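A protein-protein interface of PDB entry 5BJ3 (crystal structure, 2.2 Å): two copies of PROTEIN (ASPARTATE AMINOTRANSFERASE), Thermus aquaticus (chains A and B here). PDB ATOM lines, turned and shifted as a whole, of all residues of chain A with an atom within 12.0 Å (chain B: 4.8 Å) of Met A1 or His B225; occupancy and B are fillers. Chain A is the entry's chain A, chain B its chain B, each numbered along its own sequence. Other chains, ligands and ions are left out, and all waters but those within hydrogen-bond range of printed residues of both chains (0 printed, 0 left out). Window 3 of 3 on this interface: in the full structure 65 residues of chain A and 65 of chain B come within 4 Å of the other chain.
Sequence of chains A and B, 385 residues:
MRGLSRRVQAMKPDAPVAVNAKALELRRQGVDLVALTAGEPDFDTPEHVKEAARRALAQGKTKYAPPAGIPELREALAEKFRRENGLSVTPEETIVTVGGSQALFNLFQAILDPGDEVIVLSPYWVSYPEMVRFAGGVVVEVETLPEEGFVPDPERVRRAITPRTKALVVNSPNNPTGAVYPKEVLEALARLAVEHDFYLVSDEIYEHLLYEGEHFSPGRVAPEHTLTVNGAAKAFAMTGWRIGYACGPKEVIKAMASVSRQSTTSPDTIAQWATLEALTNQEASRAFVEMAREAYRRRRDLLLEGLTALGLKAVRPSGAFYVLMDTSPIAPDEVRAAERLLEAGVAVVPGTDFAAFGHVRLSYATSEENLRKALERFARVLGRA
Of the 13 printed residues of chain B, 5 touch a printed residue of chain A.
Hydrophobic or aromatic side chains of chain B within 4 Å of the printed part of chain A: Tyr B199 and His B225.
Hydrophobic or aromatic side chains of chain A that line the printed part of chain B: Met A1.
Among the printed residues, 9 pairs touch across the chains.
Among the printed residues, Asp or Glu carboxylates within 4 Å of a Lys or Arg side-chain nitrogen of the other chain: Arg A2 with Asp B197 (3.2 Å).
No position is printed for both chains.
Of the 9 pairs that touch across the chains among the printed residues, none has its exchanged pair printed and touching as well.
The backbone NH of Phe B198 sits at hydrogen-bond distance from the backbone carbonyl oxygen of Met A1 (3.5 Å).
The backbone carbonyl oxygen (O) of Glu B224 lies within hydrogen-bond range of the backbone NH (N) of Met A1 (3.1 Å).
NE2 of His B225 lies within hydrogen-bond range of SD of Met A1 (3.1 Å).
The guanidinium group (NH1) of Arg A2 is in salt-bridge range of the side-chain carboxylate (OD2) of Asp B197, at 3.2 Å.
N of Arg A2 sits close to OH of Tyr B199 (3.4 Å).
N of Gly A3 lies within hydrogen-bond range of OH of Tyr B199 (3.5 Å).
The side-chain carboxylate of Asp B197 sits close to the backbone carbonyl oxygen of Met A1 (2.9 Å).
Met A1 touches just these residues of chain B: Asp B197 (2.9 Å), Phe B198 (3.5 Å), Tyr B199 (3.2 Å), Glu B224 (3.1 Å) and His B225 (3.1 Å).
Printed residues of chain B within 4 Å of Arg A2: Asp B197, Phe B198 and Tyr B199.
Printed residues of chain B within 4 Å of Gly A3: Tyr B199.
No residue of chain A comes within 4 Å of Ala B193.
No residue of chain A comes within 4 Å of Val B194.
Of chain A, only Met A1 and Arg A2 come within 4 Å of Asp B197.
Of the printed residues of chain A, Phe B198 touches Met A1 (3.5 Å) and Arg A2 (3.6 Å).
Of chain A, only Met A1 (3.2 Å), Arg A2 (3.4 Å) and Gly A3 (3.5 Å) come within 4 Å of Tyr B199.
No residue of chain A comes within 4 Å of Leu B200.
No residue of chain A comes within 4 Å of Ala B222.
Pro B223 touches none of the printed residues of chain A.
Of chain A, only Met A1 (3.1 Å) comes within 4 Å of Glu B224.
His B225 touches just one residue of chain A: Met A1.
No residue of chain A comes within 4 Å of Thr B226.
No residue of chain A comes within 4 Å of Leu B227.
Met A1 touches Tyr B199.
CG of Arg A2 touches CA of Phe B198, at 3.6 Å.
The backbone carbonyl oxygen (O) of Ala B193 lies within hydrogen-bond range of the backbone NH (N) of Phe B198 (2.9 Å).
The backbone NH (N) of Leu B200 lies within hydrogen-bond range of the backbone carbonyl oxygen (O) of His B225 (2.8 Å).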
ATOM      1  N   MET A   1      13.472  -8.321  19.108  1.00  0.00           N
ATOM      2  CA  MET A   1      12.002  -8.508  18.969  1.00  0.00           C
ATOM      3  C   MET A   1      11.514  -8.065  17.602  1.00  0.00           C
ATOM      4  O   MET A   1      12.260  -7.456  16.838  1.00  0.00           O
ATOM      5  CB  MET A   1      11.241  -7.785  20.089  1.00  0.00           C
ATOM      6  CG  MET A   1      12.070  -6.776  20.860  1.00  0.00           C
ATOM      7  SD  MET A   1      12.780  -5.555  19.761  1.00  0.00           S
ATOM      8  CE  MET A   1      11.593  -4.241  19.944  1.00  0.00           C
ATOM      9  N   ARG A   2      10.259  -8.384  17.296  1.00  0.00           N
ATOM     10  CA  ARG A   2       9.651  -8.038  16.018  1.00  0.00           C
ATOM     11  C   ARG A   2       8.151  -8.259  16.136  1.00  0.00           C
ATOM     12  O   ARG A   2       7.355  -7.443  15.672  1.00  0.00           O
ATOM     13  CB  ARG A   2      10.217  -8.934  14.914  1.00  0.00           C
ATOM     14  CG  ARG A   2      10.964  -8.210  13.812  1.00  0.00           C
ATOM     15  CD  ARG A   2      10.051  -7.788  12.682  1.00  0.00           C
ATOM     16  NE  ARG A   2       8.983  -6.903  13.135  1.00  0.00           N
ATOM     17  CZ  ARG A   2       9.097  -5.583  13.240  1.00  0.00           C
ATOM     18  NH1 ARG A   2      10.237  -4.982  12.920  1.00  0.00           N
ATOM     19  NH2 ARG A   2       8.066  -4.864  13.661  1.00  0.00           N
ATOM     20  N   GLY A   3       7.778  -9.374  16.757  1.00  0.00           N
ATOM     21  CA  GLY A   3       6.374  -9.692  16.943  1.00  0.00           C
ATOM     22  C   GLY A   3       6.061 -11.162  16.770  1.00  0.00           C
ATOM     23  O   GLY A   3       6.772 -11.880  16.064  1.00  0.00           O
ATOM     24  N   LEU A   4       4.995 -11.615  17.420  1.00  0.00           N
ATOM     25  CA  LEU A   4       4.571 -13.007  17.329  1.00  0.00           C
ATOM     26  C   LEU A   4       3.693 -13.213  16.094  1.00  0.00           C
ATOM     27  O   LEU A   4       3.092 -12.268  15.583  1.00  0.00           O
ATOM     28  CB  LEU A   4       3.815 -13.414  18.596  1.00  0.00           C
ATOM     29  CG  LEU A   4       4.616 -13.337  19.901  1.00  0.00           C
ATOM     30  CD1 LEU A   4       3.717 -13.658  21.086  1.00  0.00           C
ATOM     31  CD2 LEU A   4       5.802 -14.291  19.844  1.00  0.00           C
ATOM     32  N   SER A   5       3.642 -14.446  15.607  1.00  0.00           N
ATOM     33  CA  SER A   5       2.844 -14.779  14.433  1.00  0.00           C
ATOM     34  C   SER A   5       1.353 -14.811  14.765  1.00  0.00           C
ATOM     35  O   SER A   5       0.963 -14.954  15.924  1.00  0.00           O
ATOM     36  CB  SER A   5       3.278 -16.134  13.867  1.00  0.00           C
ATOM     37  OG  SER A   5       3.062 -17.170  14.811  1.00  0.00           O
ATOM     38  N   GLN A   9      -0.923 -16.208  18.058  1.00  0.00           N
ATOM     39  CA  GLN A   9      -1.746 -15.211  18.738  1.00  0.00           C
ATOM     40  C   GLN A   9      -3.232 -15.593  18.767  1.00  0.00           C
ATOM     41  O   GLN A   9      -3.972 -15.134  19.638  1.00  0.00           O
ATOM     42  CB  GLN A   9      -1.592 -13.838  18.078  1.00  0.00           C
ATOM     43  CG  GLN A   9      -0.249 -13.170  18.325  1.00  0.00           C
ATOM     44  CD  GLN A   9      -0.186 -11.767  17.755  1.00  0.00           C
ATOM     45  OE1 GLN A   9       0.227 -11.569  16.611  1.00  0.00           O
ATOM     46  NE2 GLN A   9      -0.602 -10.787  18.546  1.00  0.00           N
ATOM     47  N   ALA B 193      20.604  -6.578  14.519  1.00  0.00           N
ATOM     48  CA  ALA B 193      19.283  -7.018  14.957  1.00  0.00           C
ATOM     49  C   ALA B 193      18.586  -5.940  15.773  1.00  0.00           C
ATOM     50  O   ALA B 193      17.381  -5.738  15.652  1.00  0.00           O
ATOM     51  CB  ALA B 193      19.398  -8.299  15.769  1.00  0.00           C
ATOM     52  N   VAL B 194      19.347  -5.267  16.626  1.00  0.00           N
ATOM     53  CA  VAL B 194      18.809  -4.194  17.457  1.00  0.00           C
ATOM     54  C   VAL B 194      18.508  -3.000  16.560  1.00  0.00           C
ATOM     55  O   VAL B 194      17.419  -2.432  16.591  1.00  0.00           O
ATOM     56  CB  VAL B 194      19.830  -3.769  18.537  1.00  0.00           C
ATOM     57  CG1 VAL B 194      19.301  -2.590  19.336  1.00  0.00           C
ATOM     58  CG2 VAL B 194      20.143  -4.938  19.456  1.00  0.00           C
ATOM     59  N   ASP B 197      15.672  -3.932  14.256  1.00  0.00           N
ATOM     60  CA  ASP B 197      14.546  -4.523  14.966  1.00  0.00           C
ATOM     61  C   ASP B 197      14.058  -5.899  14.502  1.00  0.00           C
ATOM     62  O   ASP B 197      12.941  -6.031  14.008  1.00  0.00           O
ATOM     63  CB  ASP B 197      13.371  -3.532  14.997  1.00  0.00           C
ATOM     64  CG  ASP B 197      12.274  -3.946  15.961  1.00  0.00           C
ATOM     65  OD1 ASP B 197      12.587  -4.558  16.998  1.00  0.00           O
ATOM     66  OD2 ASP B 197      11.093  -3.652  15.684  1.00  0.00           O
ATOM     67  N   PHE B 198      14.906  -6.912  14.634  1.00  0.00           N
ATOM     68  CA  PHE B 198      14.524  -8.276  14.289  1.00  0.00           C
ATOM     69  C   PHE B 198      15.123  -9.262  15.285  1.00  0.00           C
ATOM     70  O   PHE B 198      15.885  -8.870  16.169  1.00  0.00           O
ATOM     71  CB  PHE B 198      14.839  -8.640  12.823  1.00  0.00           C
ATOM     72  CG  PHE B 198      16.299  -8.561  12.441  1.00  0.00           C
ATOM     73  CD1 PHE B 198      17.199  -9.552  12.827  1.00  0.00           C
ATOM     74  CD2 PHE B 198      16.757  -7.534  11.620  1.00  0.00           C
ATOM     75  CE1 PHE B 198      18.521  -9.524  12.398  1.00  0.00           C
ATOM     76  CE2 PHE B 198      18.078  -7.497  11.187  1.00  0.00           C
ATOM     77  CZ  PHE B 198      18.962  -8.496  11.575  1.00  0.00           C
ATOM     78  N   TYR B 199      14.720 -10.526  15.191  1.00  0.00           N
ATOM     79  CA  TYR B 199      15.221 -11.549  16.101  1.00  0.00           C
ATOM     80  C   TYR B 199      16.519 -12.184  15.617  1.00  0.00           C
ATOM     81  O   TYR B 199      16.720 -12.388  14.424  1.00  0.00           O
ATOM     82  CB  TYR B 199      14.176 -12.650  16.312  1.00  0.00           C
ATOM     83  CG  TYR B 199      12.911 -12.222  17.016  1.00  0.00           C
ATOM     84  CD1 TYR B 199      12.900 -11.981  18.388  1.00  0.00           C
ATOM     85  CD2 TYR B 199      11.706 -12.116  16.317  1.00  0.00           C
ATOM     86  CE1 TYR B 199      11.738 -11.652  19.032  1.00  0.00           C
ATOM     87  CE2 TYR B 199      10.526 -11.781  16.970  1.00  0.00           C
ATOM     88  CZ  TYR B 199      10.587 -11.558  18.325  1.00  0.00           C
ATOM     89  OH  TYR B 199       9.564 -11.225  19.111  1.00  0.00           O
ATOM     90  N   LEU B 200      17.404 -12.471  16.561  1.00  0.00           N
ATOM     91  CA  LEU B 200      18.676 -13.114  16.267  1.00  0.00           C
ATOM     92  C   LEU B 200      18.548 -14.513  16.864  1.00  0.00           C
ATOM     93  O   LEU B 200      18.391 -14.662  18.074  1.00  0.00           O
ATOM     94  CB  LEU B 200      19.826 -12.341  16.927  1.00  0.00           C
ATOM     95  CG  LEU B 200      21.307 -12.657  16.645  1.00  0.00           C
ATOM     96  CD1 LEU B 200      21.800 -13.824  17.474  1.00  0.00           C
ATOM     97  CD2 LEU B 200      21.522 -12.909  15.172  1.00  0.00           C
ATOM     98  N   ALA B 222      22.291  -8.400  23.123  1.00  0.00           N
ATOM     99  CA  ALA B 222      20.897  -8.113  22.796  1.00  0.00           C
ATOM    100  C   ALA B 222      19.931  -9.167  23.336  1.00  0.00           C
ATOM    101  O   ALA B 222      19.331  -9.920  22.567  1.00  0.00           O
ATOM    102  CB  ALA B 222      20.742  -7.979  21.279  1.00  0.00           C
ATOM    103  N   PRO B 223      19.721  -9.190  24.665  1.00  0.00           N
ATOM    104  CA  PRO B 223      18.822 -10.147  25.320  1.00  0.00           C
ATOM    105  C   PRO B 223      17.358 -10.141  24.868  1.00  0.00           C
ATOM    106  O   PRO B 223      16.715 -11.187  24.847  1.00  0.00           O
ATOM    107  CB  PRO B 223      18.965  -9.792  26.804  1.00  0.00           C
ATOM    108  CG  PRO B 223      19.342  -8.347  26.784  1.00  0.00           C
ATOM    109  CD  PRO B 223      20.337  -8.299  25.662  1.00  0.00           C
ATOM    110  N   GLU B 224      16.833  -8.973  24.510  1.00  0.00           N
ATOM    111  CA  GLU B 224      15.441  -8.878  24.076  1.00  0.00           C
ATOM    112  C   GLU B 224      15.244  -9.122  22.581  1.00  0.00           C
ATOM    113  O   GLU B 224      14.129  -9.025  22.073  1.00  0.00           O
ATOM    114  CB  GLU B 224      14.846  -7.533  24.492  1.00  0.00           C
ATOM    115  CG  GLU B 224      14.821  -7.343  26.000  1.00  0.00           C
ATOM    116  CD  GLU B 224      14.222  -6.020  26.435  1.00  0.00           C
ATOM    117  OE1 GLU B 224      14.381  -5.010  25.718  1.00  0.00           O
ATOM    118  OE2 GLU B 224      13.593  -5.992  27.514  1.00  0.00           O
ATOM    119  N   HIS B 225      16.329  -9.460  21.892  1.00  0.00           N
ATOM    120  CA  HIS B 225      16.288  -9.735  20.461  1.00  0.00           C
ATOM    121  C   HIS B 225      16.777 -11.144  20.177  1.00  0.00           C
ATOM    122  O   HIS B 225      16.485 -11.702  19.124  1.00  0.00           O
ATOM    123  CB  HIS B 225      17.196  -8.768  19.698  1.00  0.00           C
ATOM    124  CG  HIS B 225      16.645  -7.385  19.575  1.00  0.00           C
ATOM    125  ND1 HIS B 225      16.604  -6.503  20.630  1.00  0.00           N
ATOM    126  CD2 HIS B 225      16.104  -6.733  18.519  1.00  0.00           C
ATOM    127  CE1 HIS B 225      16.064  -5.366  20.232  1.00  0.00           C
ATOM    128  NE2 HIS B 225      15.752  -5.482  18.956  1.00  0.00           N
ATOM    129  N   THR B 226      17.493 -11.726  21.132  1.00  0.00           N
ATOM    130  CA  THR B 226      18.072 -13.046  20.945  1.00  0.00           C
ATOM    131  C   THR B 226      17.353 -14.243  21.547  1.00  0.00           C
ATOM    132  O   THR B 226      16.936 -14.235  22.703  1.00  0.00           O
ATOM    133  CB  THR B 226      19.537 -13.063  21.429  1.00  0.00           C
ATOM    134  OG1 THR B 226      20.206 -11.891  20.949  1.00  0.00           O
ATOM    135  CG2 THR B 226      20.269 -14.290  20.904  1.00  0.00           C
ATOM    136  N   LEU B 227      17.225 -15.277  20.726  1.00  0.00           N
ATOM    137  CA  LEU B 227      16.625 -16.540  21.116  1.00  0.00           C
ATOM    138  C   LEU B 227      17.770 -17.531  21.006  1.00  0.00           C
ATOM    139  O   LEU B 227      18.266 -17.804  19.914  1.00  0.00           O
ATOM    140  CB  LEU B 227      15.493 -16.913  20.166  1.00  0.00           C
ATOM    141  CG  LEU B 227      14.192 -16.191  20.504  1.00  0.00           C
ATOM    142  CD1 LEU B 227      13.376 -15.945  19.250  1.00  0.00           C
ATOM    143  CD2 LEU B 227      13.423 -16.999  21.547  1.00  0.00           C
ATOM    144  N   PRO B 249      13.359 -13.801  25.111  1.00  0.00           N
ATOM    145  CA  PRO B 249      12.241 -12.954  25.539  1.00  0.00           C
ATOM    146  C   PRO B 249      11.071 -13.801  26.036  1.00  0.00           C
ATOM    147  O   PRO B 249      10.636 -14.739  25.366  1.00  0.00           O
ATOM    148  CB  PRO B 249      11.894 -12.190  24.265  1.00  0.00           C
ATOM    149  CG  PRO B 249      13.221 -12.044  23.603  1.00  0.00           C
ATOM    150  CD  PRO B 249      13.813 -13.419  23.760  1.00  0.00           C
